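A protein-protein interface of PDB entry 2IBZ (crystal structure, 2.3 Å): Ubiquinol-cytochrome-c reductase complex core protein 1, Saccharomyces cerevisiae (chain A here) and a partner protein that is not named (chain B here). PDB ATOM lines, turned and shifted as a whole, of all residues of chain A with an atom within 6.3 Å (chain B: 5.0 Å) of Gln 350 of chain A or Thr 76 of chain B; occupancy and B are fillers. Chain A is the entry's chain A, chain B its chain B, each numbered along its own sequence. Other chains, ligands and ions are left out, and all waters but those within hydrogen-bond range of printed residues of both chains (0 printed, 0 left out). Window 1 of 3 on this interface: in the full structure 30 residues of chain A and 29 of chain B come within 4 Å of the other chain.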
ATOM      1  N   LYS A 345       3.207  17.140   1.710  1.00  0.00           N
ATOM      2  CA  LYS A 345       3.697  17.149   3.085  1.00  0.00           C
ATOM      3  C   LYS A 345       2.985  16.077   3.881  1.00  0.00           C
ATOM      4  O   LYS A 345       3.613  15.320   4.622  1.00  0.00           O
ATOM      5  CB  LYS A 345       3.437  18.500   3.744  1.00  0.00           C
ATOM      6  CG  LYS A 345       4.293  19.636   3.227  1.00  0.00           C
ATOM      7  CD  LYS A 345       3.871  20.918   3.902  1.00  0.00           C
ATOM      8  CE  LYS A 345       4.534  22.121   3.271  1.00  0.00           C
ATOM      9  NZ  LYS A 345       4.029  23.374   3.898  1.00  0.00           N
ATOM     10  N   LEU A 346       1.671  16.004   3.703  1.00  0.00           N
ATOM     11  CA  LEU A 346       0.860  15.029   4.411  1.00  0.00           C
ATOM     12  C   LEU A 346       1.255  13.596   4.094  1.00  0.00           C
ATOM     13  O   LEU A 346       1.259  12.746   4.984  1.00  0.00           O
ATOM     14  CB  LEU A 346      -0.619  15.235   4.091  1.00  0.00           C
ATOM     15  CG  LEU A 346      -1.596  14.225   4.699  1.00  0.00           C
ATOM     16  CD1 LEU A 346      -1.683  14.418   6.203  1.00  0.00           C
ATOM     17  CD2 LEU A 346      -2.963  14.385   4.064  1.00  0.00           C
ATOM     18  N   GLN A 347       1.583  13.318   2.834  1.00  0.00           N
ATOM     19  CA  GLN A 347       1.951  11.960   2.457  1.00  0.00           C
ATOM     20  C   GLN A 347       3.391  11.659   2.821  1.00  0.00           C
ATOM     21  O   GLN A 347       3.705  10.546   3.220  1.00  0.00           O
ATOM     22  CB  GLN A 347       1.704  11.684   0.961  1.00  0.00           C
ATOM     23  CG  GLN A 347       2.799  12.181   0.011  1.00  0.00           C
ATOM     24  CD  GLN A 347       3.142  11.170  -1.086  1.00  0.00           C
ATOM     25  OE1 GLN A 347       3.174   9.957  -0.846  1.00  0.00           O
ATOM     26  NE2 GLN A 347       3.416  11.671  -2.290  1.00  0.00           N
ATOM     27  N   LEU A 348       4.259  12.654   2.681  1.00  0.00           N
ATOM     28  CA  LEU A 348       5.672  12.491   3.003  1.00  0.00           C
ATOM     29  C   LEU A 348       5.817  12.281   4.509  1.00  0.00           C
ATOM     30  O   LEU A 348       6.693  11.543   4.966  1.00  0.00           O
ATOM     31  CB  LEU A 348       6.454  13.723   2.559  1.00  0.00           C
ATOM     32  CG  LEU A 348       7.825  13.460   1.945  1.00  0.00           C
ATOM     33  CD1 LEU A 348       7.699  12.415   0.847  1.00  0.00           C
ATOM     34  CD2 LEU A 348       8.399  14.756   1.395  1.00  0.00           C
ATOM     35  N   GLY A 349       4.941  12.934   5.269  1.00  0.00           N
ATOM     36  CA  GLY A 349       4.947  12.792   6.708  1.00  0.00           C
ATOM     37  C   GLY A 349       4.523  11.383   7.063  1.00  0.00           C
ATOM     38  O   GLY A 349       5.277  10.662   7.706  1.00  0.00           O
ATOM     39  N   GLN A 350       3.351  10.967   6.588  1.00  0.00           N
ATOM     40  CA  GLN A 350       2.825   9.625   6.859  1.00  0.00           C
ATOM     41  C   GLN A 350       3.778   8.478   6.502  1.00  0.00           C
ATOM     42  O   GLN A 350       3.586   7.346   6.951  1.00  0.00           O
ATOM     43  CB  GLN A 350       1.499   9.417   6.132  1.00  0.00           C
ATOM     44  CG  GLN A 350       0.332  10.165   6.719  1.00  0.00           C
ATOM     45  CD  GLN A 350      -0.939   9.951   5.921  1.00  0.00           C
ATOM     46  OE1 GLN A 350      -1.132  10.562   4.871  1.00  0.00           O
ATOM     47  NE2 GLN A 350      -1.808   9.073   6.410  1.00  0.00           N
ATOM     48  N   LEU A 351       4.764   8.763   5.654  1.00  0.00           N
ATOM     49  CA  LEU A 351       5.751   7.760   5.257  1.00  0.00           C
ATOM     50  C   LEU A 351       6.895   7.757   6.260  1.00  0.00           C
ATOM     51  O   LEU A 351       7.155   6.750   6.919  1.00  0.00           O
ATOM     52  CB  LEU A 351       6.309   8.060   3.859  1.00  0.00           C
ATOM     53  CG  LEU A 351       5.793   7.225   2.682  1.00  0.00           C
ATOM     54  CD1 LEU A 351       6.394   7.755   1.386  1.00  0.00           C
ATOM     55  CD2 LEU A 351       6.144   5.756   2.874  1.00  0.00           C
ATOM     56  N   TYR A 352       7.556   8.906   6.378  1.00  0.00           N
ATOM     57  CA  TYR A 352       8.685   9.083   7.279  1.00  0.00           C
ATOM     58  C   TYR A 352       8.355   8.868   8.754  1.00  0.00           C
ATOM     59  O   TYR A 352       9.255   8.609   9.559  1.00  0.00           O
ATOM     60  CB  TYR A 352       9.315  10.464   7.078  1.00  0.00           C
ATOM     61  CG  TYR A 352      10.182  10.573   5.841  1.00  0.00           C
ATOM     62  CD1 TYR A 352      11.408  11.240   5.886  1.00  0.00           C
ATOM     63  CD2 TYR A 352       9.783  10.009   4.625  1.00  0.00           C
ATOM     64  CE1 TYR A 352      12.219  11.343   4.751  1.00  0.00           C
ATOM     65  CE2 TYR A 352      10.586  10.104   3.484  1.00  0.00           C
ATOM     66  CZ  TYR A 352      11.803  10.772   3.554  1.00  0.00           C
ATOM     67  OH  TYR A 352      12.602  10.870   2.437  1.00  0.00           O
ATOM     68  N   GLU A 353       7.079   8.964   9.114  1.00  0.00           N
ATOM     69  CA  GLU A 353       6.701   8.764  10.505  1.00  0.00           C
ATOM     70  C   GLU A 353       5.458   7.925  10.733  1.00  0.00           C
ATOM     71  O   GLU A 353       4.400   8.429  11.112  1.00  0.00           O
ATOM     72  CB  GLU A 353       6.618  10.096  11.272  1.00  0.00           C
ATOM     73  CG  GLU A 353       5.726  11.145  10.661  1.00  0.00           C
ATOM     74  CD  GLU A 353       5.638  12.398  11.501  1.00  0.00           C
ATOM     75  OE1 GLU A 353       4.624  12.551  12.211  1.00  0.00           O
ATOM     76  OE2 GLU A 353       6.570  13.231  11.447  1.00  0.00           O
ATOM     77  N   SER A 354       5.609   6.628  10.501  1.00  0.00           N
ATOM     78  CA  SER A 354       4.533   5.675  10.717  1.00  0.00           C
ATOM     79  C   SER A 354       4.788   5.022  12.076  1.00  0.00           C
ATOM     80  O   SER A 354       5.821   5.273  12.713  1.00  0.00           O
ATOM     81  CB  SER A 354       4.552   4.606   9.622  1.00  0.00           C
ATOM     82  OG  SER A 354       3.469   3.703   9.778  1.00  0.00           O
ATOM     83  N   LEU A 377      12.792  15.439   7.962  1.00  0.00           N
ATOM     84  CA  LEU A 377      11.442  15.722   7.489  1.00  0.00           C
ATOM     85  C   LEU A 377      11.158  17.222   7.438  1.00  0.00           C
ATOM     86  O   LEU A 377      10.504  17.704   6.513  1.00  0.00           O
ATOM     87  CB  LEU A 377      10.413  15.026   8.371  1.00  0.00           C
ATOM     88  CG  LEU A 377       9.000  15.039   7.803  1.00  0.00           C
ATOM     89  CD1 LEU A 377       8.994  14.309   6.467  1.00  0.00           C
ATOM     90  CD2 LEU A 377       8.035  14.383   8.773  1.00  0.00           C
ATOM     91  N   ILE B  12       3.028  15.191  11.988  1.00  0.00           N
ATOM     92  CA  ILE B  12       1.701  14.700  11.613  1.00  0.00           C
ATOM     93  C   ILE B  12       0.875  14.269  12.819  1.00  0.00           C
ATOM     94  O   ILE B  12       1.264  13.364  13.555  1.00  0.00           O
ATOM     95  CB  ILE B  12       1.800  13.485  10.632  1.00  0.00           C
ATOM     96  CG1 ILE B  12       2.581  13.867   9.372  1.00  0.00           C
ATOM     97  CG2 ILE B  12       0.416  12.967  10.272  1.00  0.00           C
ATOM     98  CD1 ILE B  12       1.965  14.996   8.576  1.00  0.00           C
ATOM     99  N   SER B  13      -0.275  14.906  13.005  1.00  0.00           N
ATOM    100  CA  SER B  13      -1.169  14.569  14.110  1.00  0.00           C
ATOM    101  C   SER B  13      -2.320  13.731  13.568  1.00  0.00           C
ATOM    102  O   SER B  13      -2.531  13.668  12.359  1.00  0.00           O
ATOM    103  CB  SER B  13      -1.710  15.841  14.764  1.00  0.00           C
ATOM    104  OG  SER B  13      -0.656  16.694  15.182  1.00  0.00           O
ATOM    105  N   THR B  14      -3.065  13.079  14.456  1.00  0.00           N
ATOM    106  CA  THR B  14      -4.183  12.256  14.019  1.00  0.00           C
ATOM    107  C   THR B  14      -5.329  12.157  15.018  1.00  0.00           C
ATOM    108  O   THR B  14      -5.330  11.316  15.917  1.00  0.00           O
ATOM    109  CB  THR B  14      -3.715  10.838  13.533  1.00  0.00           C
ATOM    110  OG1 THR B  14      -4.782   9.889  13.660  1.00  0.00           O
ATOM    111  CG2 THR B  14      -2.501  10.353  14.309  1.00  0.00           C
ATOM    112  N   GLY B  59      -4.009  20.502   4.296  1.00  0.00           N
ATOM    113  CA  GLY B  59      -3.083  19.393   4.266  1.00  0.00           C
ATOM    114  C   GLY B  59      -3.516  18.287   5.195  1.00  0.00           C
ATOM    115  O   GLY B  59      -2.751  17.884   6.064  1.00  0.00           O
ATOM    116  N   GLY B  60      -4.735  17.792   5.012  1.00  0.00           N
ATOM    117  CA  GLY B  60      -5.233  16.720   5.854  1.00  0.00           C
ATOM    118  C   GLY B  60      -6.384  15.980   5.206  1.00  0.00           C
ATOM    119  O   GLY B  60      -7.082  16.546   4.368  1.00  0.00           O
ATOM    120  N   THR B  61      -6.579  14.714   5.578  1.00  0.00           N
ATOM    121  CA  THR B  61      -7.663  13.910   5.017  1.00  0.00           C
ATOM    122  C   THR B  61      -8.546  13.303   6.100  1.00  0.00           C
ATOM    123  O   THR B  61      -8.184  13.280   7.273  1.00  0.00           O
ATOM    124  CB  THR B  61      -7.131  12.757   4.110  1.00  0.00           C
ATOM    125  OG1 THR B  61      -6.404  11.808   4.900  1.00  0.00           O
ATOM    126  CG2 THR B  61      -6.224  13.301   3.011  1.00  0.00           C
ATOM    127  N   LYS B  74     -11.690   9.071  11.858  1.00  0.00           N
ATOM    128  CA  LYS B  74     -10.307   9.533  11.991  1.00  0.00           C
ATOM    129  C   LYS B  74      -9.980  10.693  11.049  1.00  0.00           C
ATOM    130  O   LYS B  74     -10.622  10.862  10.018  1.00  0.00           O
ATOM    131  CB  LYS B  74      -9.365   8.348  11.741  1.00  0.00           C
ATOM    132  CG  LYS B  74      -7.888   8.605  11.994  1.00  0.00           C
ATOM    133  CD  LYS B  74      -7.059   7.370  11.634  1.00  0.00           C
ATOM    134  CE  LYS B  74      -5.566   7.676  11.613  1.00  0.00           C
ATOM    135  NZ  LYS B  74      -4.744   6.513  11.154  1.00  0.00           N
ATOM    136  N   ALA B  75      -8.978  11.491  11.414  1.00  0.00           N
ATOM    137  CA  ALA B  75      -8.553  12.635  10.609  1.00  0.00           C
ATOM    138  C   ALA B  75      -7.054  12.856  10.762  1.00  0.00           C
ATOM    139  O   ALA B  75      -6.580  13.224  11.833  1.00  0.00           O
ATOM    140  CB  ALA B  75      -9.304  13.888  11.023  1.00  0.00           C
ATOM    141  N   THR B  76      -6.315  12.636   9.683  1.00  0.00           N
ATOM    142  CA  THR B  76      -4.868  12.791   9.679  1.00  0.00           C
ATOM    143  C   THR B  76      -4.548  14.147   9.070  1.00  0.00           C
ATOM    144  O   THR B  76      -5.114  14.503   8.043  1.00  0.00           O
ATOM    145  CB  THR B  76      -4.243  11.674   8.853  1.00  0.00           C
ATOM    146  OG1 THR B  76      -4.813  10.423   9.260  1.00  0.00           O
ATOM    147  CG2 THR B  76      -2.743  11.641   9.041  1.00  0.00           C
ATOM    148  N   PHE B  77      -3.616  14.887   9.670  1.00  0.00           N
ATOM    149  CA  PHE B  77      -3.293  16.231   9.186  1.00  0.00           C
ATOM    150  C   PHE B  77      -1.998  16.778   9.749  1.00  0.00           C
ATOM    151  O   PHE B  77      -1.322  16.113  10.526  1.00  0.00           O
ATOM    152  CB  PHE B  77      -4.404  17.182   9.615  1.00  0.00           C
ATOM    153  CG  PHE B  77      -4.691  17.136  11.096  1.00  0.00           C
ATOM    154  CD1 PHE B  77      -4.132  18.077  11.961  1.00  0.00           C
ATOM    155  CD2 PHE B  77      -5.495  16.130  11.632  1.00  0.00           C
ATOM    156  CE1 PHE B  77      -4.370  18.011  13.343  1.00  0.00           C
ATOM    157  CE2 PHE B  77      -5.736  16.058  13.006  1.00  0.00           C
ATOM    158  CZ  PHE B  77      -5.173  16.999  13.863  1.00  0.00           C
ATOM    159  N   LEU B  78      -1.684  18.014   9.372  1.00  0.00           N
ATOM    160  CA  LEU B  78      -0.487  18.694   9.861  1.00  0.00           C
ATOM    161  C   LEU B  78      -0.810  19.253  11.250  1.00  0.00           C
ATOM    162  O   LEU B  78      -1.841  19.903  11.443  1.00  0.00           O
ATOM    163  CB  LEU B  78      -0.070  19.820   8.912  1.00  0.00           C
ATOM    164  CG  LEU B  78       0.136  19.441   7.442  1.00  0.00           C
ATOM    165  CD1 LEU B  78       0.622  20.652   6.649  1.00  0.00           C
ATOM    166  CD2 LEU B  78       1.130  18.302   7.329  1.00  0.00           C
ATOM    167  N   TYR B  85      -9.990  20.376  12.299  1.00  0.00           N
ATOM    168  CA  TYR B  85     -10.437  18.990  12.262  1.00  0.00           C
ATOM    169  C   TYR B  85     -11.318  18.579  13.438  1.00  0.00           C
ATOM    170  O   TYR B  85     -12.120  17.640  13.319  1.00  0.00           O
ATOM    171  CB  TYR B  85      -9.234  18.063  12.104  1.00  0.00           C
ATOM    172  CG  TYR B  85      -8.428  18.403  10.871  1.00  0.00           C
ATOM    173  CD1 TYR B  85      -7.448  19.390  10.915  1.00  0.00           C
ATOM    174  CD2 TYR B  85      -8.688  17.783   9.640  1.00  0.00           C
ATOM    175  CE1 TYR B  85      -6.749  19.760   9.770  1.00  0.00           C
ATOM    176  CE2 TYR B  85      -7.991  18.145   8.487  1.00  0.00           C
ATOM    177  CZ  TYR B  85      -7.026  19.134   8.562  1.00  0.00           C
ATOM    178  OH  TYR B  85      -6.325  19.513   7.441  1.00  0.00           O
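The backbone NH (N) of Ile 12 of chain B lies within hydrogen-bond range of the side-chain carboxylate (OE1) of Glu 353 of chain A.
The side-chain amide oxygen of Gln 350 of chain A lies close to the backbone carbonyl oxygen of Leu 346 of chain A, at 3.2 Å.
The backbone NH (N) of Ser 13 of chain B sits at hydrogen-bond distance from the backbone carbonyl oxygen (O) of Phe 77 of chain B.
The backbone NH (N) of Leu 78 of chain B is in hydrogen-bond range of the backbone carbonyl oxygen (O) of Gly 59 of chain B, at 3.5 Å.
The side-chain hydroxyl of Tyr 85 of chain B lies within hydrogen-bond range of the backbone NH of Gly 60 of chain B (3.4 Å).
The backbone carbonyl oxygen of Thr 76 of chain B lies within hydrogen-bond range of the backbone NH of Thr 61 of chain B.
Among the printed residues, pairs that only touch across the chains: Leu 346 of chain A with Thr 61 of chain B, Leu 346 of chain A with Gly 59 of chain B, Leu 346 of chain A with Gly 60 of chain B, Gly 349 of chain A with Ile 12 of chain B, Gln 350 of chain A with Thr 76 of chain B, Leu 346 of chain A with Phe 77 of chain B and Leu 346 of chain A with Thr 76 of chain B.
Printed residues of chain B within 4 Å of Leu 346 of chain A: Gly 59 (3.6 Å), Gly 60 (3.7 Å), Thr 61 (3.6 Å), Thr 76 (3.9 Å) and Phe 77 (3.8 Å).
Gln 350 of chain A touches just one residue of chain B: Thr 76 (3.8 Å).
Printed residues of chain B within 4 Å of Glu 353 of chain A: Ile 12 (3.1 Å).
Of the printed residues of chain A, Gly 59 of chain B touches Leu 346 (3.6 Å).
Of the printed residues of chain A, Gly 60 of chain B touches Leu 346 (3.7 Å).
Of the printed residues of chain A, Thr 76 of chain B touches Leu 346 and Gln 350.
Of the printed residues of chain A, Phe 77 of chain B touches Leu 346 (3.8 Å).
The nearest printed residue of chain B that does not touch Gly 349 of chain A is Leu 78 of chain B (6.7 Å).
Hydrophobic or aromatic side chains of chain B that line the printed part of chain A: Ile 12.
Along chain B the printed residues that touch a printed residue of chain A span positions 12 to 77.
Hydrophobic or aromatic side chains of chain A within 4 Å of the printed part of chain B: Leu 346.
Among the printed residues, no Asp or Glu carboxylate lies within 4 Å of a Lys or Arg side-chain nitrogen of the other chain.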
